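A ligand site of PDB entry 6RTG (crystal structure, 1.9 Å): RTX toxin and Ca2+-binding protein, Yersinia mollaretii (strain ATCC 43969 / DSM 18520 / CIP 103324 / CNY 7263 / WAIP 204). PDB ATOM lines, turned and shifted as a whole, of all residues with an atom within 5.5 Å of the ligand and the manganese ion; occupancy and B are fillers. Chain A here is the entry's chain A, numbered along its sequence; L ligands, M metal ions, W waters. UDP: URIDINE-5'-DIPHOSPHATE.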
ATOM      1  N   VAL A  23     -11.366 -10.838  21.856  1.00  0.00           N
ATOM      2  CA  VAL A  23     -12.804 -10.843  21.611  1.00  0.00           C
ATOM      3  C   VAL A  23     -13.291 -12.291  21.661  1.00  0.00           C
ATOM      4  O   VAL A  23     -12.703 -13.176  21.024  1.00  0.00           O
ATOM      5  CB  VAL A  23     -13.159 -10.195  20.257  1.00  0.00           C
ATOM      6  CG1 VAL A  23     -14.642 -10.393  19.903  1.00  0.00           C
ATOM      7  CG2 VAL A  23     -12.838  -8.696  20.267  1.00  0.00           C
ATOM      8  N   TRP A  24     -14.364 -12.539  22.414  1.00  0.00           N
ATOM      9  CA  TRP A  24     -15.056 -13.813  22.253  1.00  0.00           C
ATOM     10  C   TRP A  24     -16.542 -13.565  22.427  1.00  0.00           C
ATOM     11  O   TRP A  24     -17.002 -13.302  23.544  1.00  0.00           O
ATOM     12  CB  TRP A  24     -14.564 -14.897  23.204  1.00  0.00           C
ATOM     13  CG  TRP A  24     -15.135 -16.199  22.735  1.00  0.00           C
ATOM     14  CD1 TRP A  24     -16.349 -16.742  23.087  1.00  0.00           C
ATOM     15  CD2 TRP A  24     -14.578 -17.062  21.748  1.00  0.00           C
ATOM     16  NE1 TRP A  24     -16.551 -17.910  22.399  1.00  0.00           N
ATOM     17  CE2 TRP A  24     -15.487 -18.140  21.568  1.00  0.00           C
ATOM     18  CE3 TRP A  24     -13.389 -17.057  21.010  1.00  0.00           C
ATOM     19  CZ2 TRP A  24     -15.236 -19.183  20.691  1.00  0.00           C
ATOM     20  CZ3 TRP A  24     -13.142 -18.108  20.128  1.00  0.00           C
ATOM     21  CH2 TRP A  24     -14.066 -19.156  19.976  1.00  0.00           C
ATOM     22  N   ILE A  25     -17.293 -13.700  21.334  1.00  0.00           N
ATOM     23  CA  ILE A  25     -18.726 -13.445  21.289  1.00  0.00           C
ATOM     24  C   ILE A  25     -19.467 -14.664  20.760  1.00  0.00           C
ATOM     25  O   ILE A  25     -18.889 -15.551  20.113  1.00  0.00           O
ATOM     26  CB  ILE A  25     -19.038 -12.206  20.414  1.00  0.00           C
ATOM     27  CG1 ILE A  25     -18.291 -12.344  19.078  1.00  0.00           C
ATOM     28  CG2 ILE A  25     -18.601 -10.925  21.132  1.00  0.00           C
ATOM     29  CD1 ILE A  25     -18.734 -11.407  18.030  1.00  0.00           C
ATOM     30  N   GLY A  26     -20.763 -14.701  21.024  1.00  0.00           N
ATOM     31  CA  GLY A  26     -21.649 -15.708  20.493  1.00  0.00           C
ATOM     32  C   GLY A  26     -21.926 -16.862  21.421  1.00  0.00           C
ATOM     33  O   GLY A  26     -22.890 -17.607  21.190  1.00  0.00           O
ATOM     34  N   ALA A  61     -24.011 -18.957  18.770  1.00  0.00           N
ATOM     35  CA  ALA A  61     -23.343 -20.182  18.310  1.00  0.00           C
ATOM     36  C   ALA A  61     -24.279 -21.374  18.403  1.00  0.00           C
ATOM     37  O   ALA A  61     -24.302 -22.227  17.505  1.00  0.00           O
ATOM     38  CB  ALA A  61     -22.065 -20.422  19.120  1.00  0.00           C
ATOM     39  N   LEU A 191     -19.240 -15.561  13.422  1.00  0.00           N
ATOM     40  CA  LEU A 191     -18.748 -14.888  14.618  1.00  0.00           C
ATOM     41  C   LEU A 191     -17.326 -14.372  14.438  1.00  0.00           C
ATOM     42  O   LEU A 191     -16.943 -13.376  15.066  1.00  0.00           O
ATOM     43  CB  LEU A 191     -18.844 -15.827  15.826  1.00  0.00           C
ATOM     44  CG  LEU A 191     -20.277 -16.219  16.200  1.00  0.00           C
ATOM     45  CD1 LEU A 191     -20.329 -17.262  17.307  1.00  0.00           C
ATOM     46  CD2 LEU A 191     -21.081 -14.992  16.603  1.00  0.00           C
ATOM     47  N   ALA A 192     -16.521 -15.031  13.600  1.00  0.00           N
ATOM     48  CA  ALA A 192     -15.202 -14.488  13.286  1.00  0.00           C
ATOM     49  C   ALA A 192     -15.333 -13.155  12.544  1.00  0.00           C
ATOM     50  O   ALA A 192     -14.599 -12.208  12.828  1.00  0.00           O
ATOM     51  CB  ALA A 192     -14.392 -15.501  12.472  1.00  0.00           C
ATOM     52  N   SER A 195     -16.263 -10.471  14.877  1.00  0.00           N
ATOM     53  CA  SER A 195     -15.049 -10.118  15.606  1.00  0.00           C
ATOM     54  C   SER A 195     -14.118  -9.257  14.762  1.00  0.00           C
ATOM     55  O   SER A 195     -13.386  -8.423  15.315  1.00  0.00           O
ATOM     56  CB  SER A 195     -14.336 -11.400  16.060  1.00  0.00           C
ATOM     57  OG  SER A 195     -13.106 -11.112  16.687  1.00  0.00           O
ATOM     58  N   ARG A 199     -12.846  -5.812  16.884  1.00  0.00           N
ATOM     59  CA  ARG A 199     -11.439  -5.528  17.175  1.00  0.00           C
ATOM     60  C   ARG A 199     -11.062  -4.120  16.735  1.00  0.00           C
ATOM     61  O   ARG A 199     -10.261  -3.446  17.401  1.00  0.00           O
ATOM     62  CB  ARG A 199     -10.542  -6.568  16.511  1.00  0.00           C
ATOM     63  CG  ARG A 199     -10.484  -6.483  14.981  1.00  0.00           C
ATOM     64  CD  ARG A 199      -9.842  -7.757  14.407  1.00  0.00           C
ATOM     65  NE  ARG A 199     -10.658  -8.923  14.726  1.00  0.00           N
ATOM     66  CZ  ARG A 199     -10.356 -10.166  14.361  1.00  0.00           C
ATOM     67  NH1 ARG A 199      -9.247 -10.393  13.664  1.00  0.00           N
ATOM     68  NH2 ARG A 199     -11.165 -11.150  14.708  1.00  0.00           N
ATOM     69  N   TYR A 210      -4.450  -5.767  19.833  1.00  0.00           N
ATOM     70  CA  TYR A 210      -5.471  -6.800  19.652  1.00  0.00           C
ATOM     71  C   TYR A 210      -4.835  -8.078  19.114  1.00  0.00           C
ATOM     72  O   TYR A 210      -3.997  -8.019  18.197  1.00  0.00           O
ATOM     73  CB  TYR A 210      -6.599  -6.336  18.686  1.00  0.00           C
ATOM     74  CG  TYR A 210      -7.479  -7.519  18.331  1.00  0.00           C
ATOM     75  CD1 TYR A 210      -8.551  -7.883  19.154  1.00  0.00           C
ATOM     76  CD2 TYR A 210      -7.203  -8.322  17.226  1.00  0.00           C
ATOM     77  CE1 TYR A 210      -9.323  -8.998  18.870  1.00  0.00           C
ATOM     78  CE2 TYR A 210      -7.958  -9.435  16.945  1.00  0.00           C
ATOM     79  CZ  TYR A 210      -9.016  -9.769  17.769  1.00  0.00           C
ATOM     80  OH  TYR A 210      -9.768 -10.890  17.477  1.00  0.00           O
ATOM     81  N   ILE A 211      -5.269  -9.236  19.631  1.00  0.00           N
ATOM     82  CA  ILE A 211      -4.889 -10.547  19.115  1.00  0.00           C
ATOM     83  C   ILE A 211      -6.098 -11.474  19.073  1.00  0.00           C
ATOM     84  O   ILE A 211      -6.943 -11.463  19.983  1.00  0.00           O
ATOM     85  CB  ILE A 211      -3.769 -11.194  19.966  1.00  0.00           C
ATOM     86  CG1 ILE A 211      -4.288 -11.395  21.386  1.00  0.00           C
ATOM     87  CG2 ILE A 211      -2.527 -10.324  19.968  1.00  0.00           C
ATOM     88  CD1 ILE A 211      -3.245 -11.744  22.382  1.00  0.00           C
ATOM     89  N   ASP A 212      -6.190 -12.311  18.030  1.00  0.00           N
ATOM     90  CA  ASP A 212      -7.119 -13.434  18.015  1.00  0.00           C
ATOM     91  C   ASP A 212      -6.805 -14.384  19.160  1.00  0.00           C
ATOM     92  O   ASP A 212      -5.647 -14.545  19.557  1.00  0.00           O
ATOM     93  CB  ASP A 212      -7.029 -14.206  16.687  1.00  0.00           C
ATOM     94  CG  ASP A 212      -7.868 -13.589  15.564  1.00  0.00           C
ATOM     95  OD1 ASP A 212      -8.501 -12.546  15.781  1.00  0.00           O
ATOM     96  OD2 ASP A 212      -7.856 -14.151  14.449  1.00  0.00           O
ATOM     97  N   THR A 213      -7.857 -15.035  19.694  1.00  0.00           N
ATOM     98  CA  THR A 213      -7.687 -15.867  20.894  1.00  0.00           C
ATOM     99  C   THR A 213      -6.951 -17.169  20.619  1.00  0.00           C
ATOM    100  O   THR A 213      -6.621 -17.876  21.584  1.00  0.00           O
ATOM    101  CB  THR A 213      -9.052 -16.201  21.528  1.00  0.00           C
ATOM    102  OG1 THR A 213      -9.871 -16.923  20.582  1.00  0.00           O
ATOM    103  CG2 THR A 213      -9.770 -14.921  21.937  1.00  0.00           C
ATOM    104  N   ASP A 214      -6.674 -17.514  19.367  1.00  0.00           N
ATOM    105  CA  ASP A 214      -5.923 -18.729  19.081  1.00  0.00           C
ATOM    106  C   ASP A 214      -4.452 -18.440  18.789  1.00  0.00           C
ATOM    107  O   ASP A 214      -3.750 -19.324  18.271  1.00  0.00           O
ATOM    108  CB  ASP A 214      -6.574 -19.502  17.918  1.00  0.00           C
ATOM    109  CG  ASP A 214      -6.607 -18.708  16.615  1.00  0.00           C
ATOM    110  OD1 ASP A 214      -7.165 -19.226  15.628  1.00  0.00           O
ATOM    111  OD2 ASP A 214      -6.077 -17.586  16.546  1.00  0.00           O
ATOM    112  N   GLU A 427      -4.116 -24.237  17.814  1.00  0.00           N
ATOM    113  CA  GLU A 427      -5.503 -23.803  17.632  1.00  0.00           C
ATOM    114  C   GLU A 427      -5.725 -22.998  16.349  1.00  0.00           C
ATOM    115  O   GLU A 427      -6.845 -23.021  15.843  1.00  0.00           O
ATOM    116  CB  GLU A 427      -5.976 -23.005  18.836  1.00  0.00           C
ATOM    117  CG  GLU A 427      -6.371 -23.892  20.022  1.00  0.00           C
ATOM    118  CD  GLU A 427      -7.535 -24.832  19.694  1.00  0.00           C
ATOM    119  OE1 GLU A 427      -8.558 -24.351  19.186  1.00  0.00           O
ATOM    120  OE2 GLU A 427      -7.413 -26.046  19.938  1.00  0.00           O
ATOM    121  N   GLU A 428      -4.710 -22.323  15.806  1.00  0.00           N
ATOM    122  CA  GLU A 428      -4.912 -21.539  14.586  1.00  0.00           C
ATOM    123  C   GLU A 428      -5.311 -22.402  13.396  1.00  0.00           C
ATOM    124  O   GLU A 428      -5.990 -21.906  12.480  1.00  0.00           O
ATOM    125  CB  GLU A 428      -3.663 -20.705  14.263  1.00  0.00           C
ATOM    126  CG  GLU A 428      -3.483 -20.230  12.798  1.00  0.00           C
ATOM    127  CD  GLU A 428      -4.574 -19.296  12.259  1.00  0.00           C
ATOM    128  OE1 GLU A 428      -5.570 -18.987  12.931  1.00  0.00           O
ATOM    129  OE2 GLU A 428      -4.423 -18.832  11.110  1.00  0.00           O
ATOM    130  N   PHE A 430      -7.529 -24.694  13.423  1.00  0.00           N
ATOM    131  CA  PHE A 430      -8.941 -25.097  13.573  1.00  0.00           C
ATOM    132  C   PHE A 430      -9.821 -23.855  13.434  1.00  0.00           C
ATOM    133  O   PHE A 430     -10.067 -23.146  14.410  1.00  0.00           O
ATOM    134  CB  PHE A 430      -9.187 -25.791  14.905  1.00  0.00           C
ATOM    135  CG  PHE A 430      -8.439 -27.089  15.063  1.00  0.00           C
ATOM    136  CD1 PHE A 430      -7.138 -27.092  15.540  1.00  0.00           C
ATOM    137  CD2 PHE A 430      -9.026 -28.297  14.709  1.00  0.00           C
ATOM    138  CE1 PHE A 430      -6.440 -28.290  15.677  1.00  0.00           C
ATOM    139  CE2 PHE A 430      -8.334 -29.489  14.840  1.00  0.00           C
ATOM    140  CZ  PHE A 430      -7.039 -29.486  15.312  1.00  0.00           C
ATOM    141  N   SER A 431     -10.322 -23.624  12.221  1.00  0.00           N
ATOM    142  CA  SER A 431     -11.170 -22.454  11.956  1.00  0.00           C
ATOM    143  C   SER A 431     -12.592 -22.678  12.446  1.00  0.00           C
ATOM    144  O   SER A 431     -13.147 -23.777  12.317  1.00  0.00           O
ATOM    145  CB  SER A 431     -11.193 -22.140  10.450  1.00  0.00           C
ATOM    146  OG  SER A 431     -12.001 -20.992  10.211  1.00  0.00           O
ATOM    147  N   SER A 432     -13.192 -21.635  13.016  1.00  0.00           N
ATOM    148  CA  SER A 432     -14.597 -21.696  13.398  1.00  0.00           C
ATOM    149  C   SER A 432     -15.547 -21.567  12.219  1.00  0.00           C
ATOM    150  O   SER A 432     -16.757 -21.804  12.381  1.00  0.00           O
ATOM    151  CB  SER A 432     -14.911 -20.597  14.413  1.00  0.00           C
ATOM    152  OG  SER A 432     -14.658 -19.314  13.839  1.00  0.00           O
ATOM    153  N   TRP A 433     -15.066 -21.192  11.038  1.00  0.00           N
ATOM    154  CA  TRP A 433     -15.954 -20.937   9.913  1.00  0.00           C
ATOM    155  C   TRP A 433     -15.423 -21.427   8.575  1.00  0.00           C
ATOM    156  O   TRP A 433     -16.231 -21.804   7.721  1.00  0.00           O
ATOM    157  CB  TRP A 433     -16.259 -19.446   9.789  1.00  0.00           C
ATOM    158  CG  TRP A 433     -15.039 -18.668   9.347  1.00  0.00           C
ATOM    159  CD1 TRP A 433     -13.991 -18.264  10.135  1.00  0.00           C
ATOM    160  CD2 TRP A 433     -14.744 -18.226   8.016  1.00  0.00           C
ATOM    161  NE1 TRP A 433     -13.063 -17.597   9.370  1.00  0.00           N
ATOM    162  CE2 TRP A 433     -13.510 -17.554   8.063  1.00  0.00           C
ATOM    163  CE3 TRP A 433     -15.415 -18.329   6.792  1.00  0.00           C
ATOM    164  CZ2 TRP A 433     -12.914 -16.990   6.935  1.00  0.00           C
ATOM    165  CZ3 TRP A 433     -14.830 -17.773   5.665  1.00  0.00           C
ATOM    166  CH2 TRP A 433     -13.595 -17.105   5.742  1.00  0.00           C
ATOM    167  N   SER A 434     -14.119 -21.444   8.332  1.00  0.00           N
ATOM    168  CA  SER A 434     -13.600 -21.756   7.001  1.00  0.00           C
ATOM    169  C   SER A 434     -13.541 -23.268   6.780  1.00  0.00           C
ATOM    170  O   SER A 434     -13.320 -24.054   7.716  1.00  0.00           O
ATOM    171  CB  SER A 434     -12.208 -21.150   6.821  1.00  0.00           C
ATOM    172  OG  SER A 434     -11.805 -21.199   5.462  1.00  0.00           O
HETATM  173  N1  UDP L   1     -14.732 -15.659  17.468  1.00  0.00           N
HETATM  174  C2  UDP L   1     -15.675 -15.452  18.454  1.00  0.00           C
HETATM  175  N3  UDP L   1     -16.572 -16.475  18.636  1.00  0.00           N
HETATM  176  C4  UDP L   1     -16.618 -17.662  17.951  1.00  0.00           C
HETATM  177  C5  UDP L   1     -15.605 -17.814  16.937  1.00  0.00           C
HETATM  178  C6  UDP L   1     -14.713 -16.829  16.737  1.00  0.00           C
HETATM  179  O2  UDP L   1     -15.714 -14.432  19.133  1.00  0.00           O
HETATM  180  O4  UDP L   1     -17.487 -18.494  18.238  1.00  0.00           O
HETATM  181  C1' UDP L   1     -13.746 -14.587  17.251  1.00  0.00           C
HETATM  182  C2' UDP L   1     -12.589 -14.637  18.258  1.00  0.00           C
HETATM  183  O2' UDP L   1     -12.190 -13.293  18.518  1.00  0.00           O
HETATM  184  C3' UDP L   1     -11.550 -15.424  17.459  1.00  0.00           C
HETATM  185  C4' UDP L   1     -11.751 -14.842  16.061  1.00  0.00           C
HETATM  186  O4' UDP L   1     -13.184 -14.727  15.954  1.00  0.00           O
HETATM  187  O3' UDP L   1     -10.244 -15.218  17.960  1.00  0.00           O
HETATM  188  C5' UDP L   1     -11.189 -15.626  14.907  1.00  0.00           C
HETATM  189  O5' UDP L   1     -11.749 -16.965  14.898  1.00  0.00           O
HETATM  190  PA  UDP L   1     -11.076 -18.137  14.068  1.00  0.00           P
HETATM  191  O1A UDP L   1      -9.701 -18.292  14.591  1.00  0.00           O
HETATM  192  O2A UDP L   1     -11.954 -19.373  14.075  1.00  0.00           O
HETATM  193  O3A UDP L   1     -11.062 -17.605  12.562  1.00  0.00           O
HETATM  194  PB  UDP L   1      -9.983 -17.881  11.440  1.00  0.00           P
HETATM  195  O1B UDP L   1      -8.573 -17.493  11.926  1.00  0.00           O
HETATM  196  O2B UDP L   1     -10.487 -17.088  10.281  1.00  0.00           O
HETATM  197  O3B UDP L   1     -10.118 -19.382  11.176  1.00  0.00           O
HETATM  198 MN    MN M   1      -7.633 -18.333  13.627  1.00  0.00          MN
HETATM  199  O   HOH W   1     -18.986 -18.609  20.691  1.00  0.00           O
HETATM  200  O   HOH W   2      -9.543 -12.184  20.083  1.00  0.00           O
HETATM  201  O   HOH W   3      -9.234 -17.449  17.169  1.00  0.00           O
HETATM  202  O   HOH W   4      -8.275 -20.392  12.848  1.00  0.00           O
HETATM  203  O   HOH W   5     -12.045 -20.326  16.808  1.00  0.00           O
HETATM  204  O   HOH W   6      -6.707 -16.397  14.208  1.00  0.00           O
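NE1 of Trp 433 sits at hydrogen-bond distance from O2B of the ligand (2.8 Å). An oxygen (O2') of the ligand is in hydrogen-bond range of the side-chain hydroxyl of Ser 195, at 3.0 Å. The side-chain hydroxyl (OG) of Ser 431 lies within hydrogen-bond range of an oxygen (O3B) of the ligand. OG1 of Thr 213 lies within hydrogen-bond range of O3' of the ligand (3.1 Å). An oxygen (O3') of the ligand is in hydrogen-bond range of the backbone NH (N) of Thr 213 (3.0 Å). The backbone carbonyl oxygen (O) of Ile 25 is in hydrogen-bond range of a nitrogen (N3) of the ligand, at 2.9 Å. An oxygen (O2') of the ligand lies within hydrogen-bond range of the backbone carbonyl oxygen (O) of Val 23 (2.6 Å). The side-chain hydroxyl of Ser 432 lies within hydrogen-bond range of an oxygen (O2A) of the ligand. An oxygen (O2) of the ligand is in hydrogen-bond range of the backbone NH (N) of Ile 25. O2A of the ligand lies within hydrogen-bond range of N of Ser 432 (2.8 Å).
The side-chain hydroxyl (OH) of Tyr 210 sits at hydrogen-bond distance from the side-chain carboxylate (OD1) of Asp 212 (2.7 Å). The side-chain hydroxyl (OG) of Ser 431 sits at hydrogen-bond distance from the backbone NH (N) of Trp 433. The side-chain hydroxyl (OG) of Ser 431 sits at hydrogen-bond distance from the backbone NH (N) of Ser 434. OG of Ser 195 is in hydrogen-bond range of OH of Tyr 210 (3.4 Å). The guanidinium group (NH1) of Arg 199 is in salt-bridge range of the side-chain carboxylate (OD1) of Asp 212, at 3.1 Å. NH2 of Arg 199 is in hydrogen-bond range of OG of Ser 195 (2.8 Å). The guanidinium group of Arg 199 lies within hydrogen-bond range of the side-chain hydroxyl of Tyr 210 (3.1 Å).
The manganese ion is bound by an oxygen (O1B) of the ligand, water W6, the side-chain carboxylate (OD1) of Asp 214, the side-chain carboxylate (OE1) of Glu 428, an oxygen (O1A) of the ligand and water W4.
CA of Trp 24 touches O2 of the ligand (3.2 Å). CD1 of Leu 191 touches O4 of the ligand (3.2 Å). Ala 192 touches the ligand (CA to O4', 3.4 Å). Arg 199 touches the ligand. OH of Tyr 210 touches O2' of the ligand, at 3.6 Å. Asp 212 touches the ligand.
Water W6 bridges the side-chain carboxylate (OD2) of Asp 212 (2.5 Å) and the side-chain carboxylate (OD2) of Asp 214 (2.7 Å). Water W4 lies within hydrogen-bond range of an oxygen (O3B) of the ligand (2.7 Å) and the backbone carbonyl oxygen of Glu 428 (2.8 Å). Water W3 bridges O3' of the ligand and OD2 of Asp 214. Water W1 lies within hydrogen-bond range of an oxygen (O4) of the ligand (2.9 Å), the indole nitrogen of Trp 24 (3.1 Å) and the backbone carbonyl oxygen of Ile 25 (3.1 Å). Water W2 lies within hydrogen-bond range of the backbone carbonyl oxygen (O) of Ile 211 (2.7 Å), the backbone NH (N) of Val 23 (2.9 Å), the side-chain hydroxyl (OH) of Tyr 210 (2.9 Å), an oxygen (O2') of the ligand (3.3 Å) and the backbone NH (N) of Thr 213 (3.3 Å).
Two residues have an atom within 4 Å of the manganese ion: Asp 214 and Glu 428. The nearest printed residue that does not touch the manganese ion is Asp 212 (4.3 Å).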
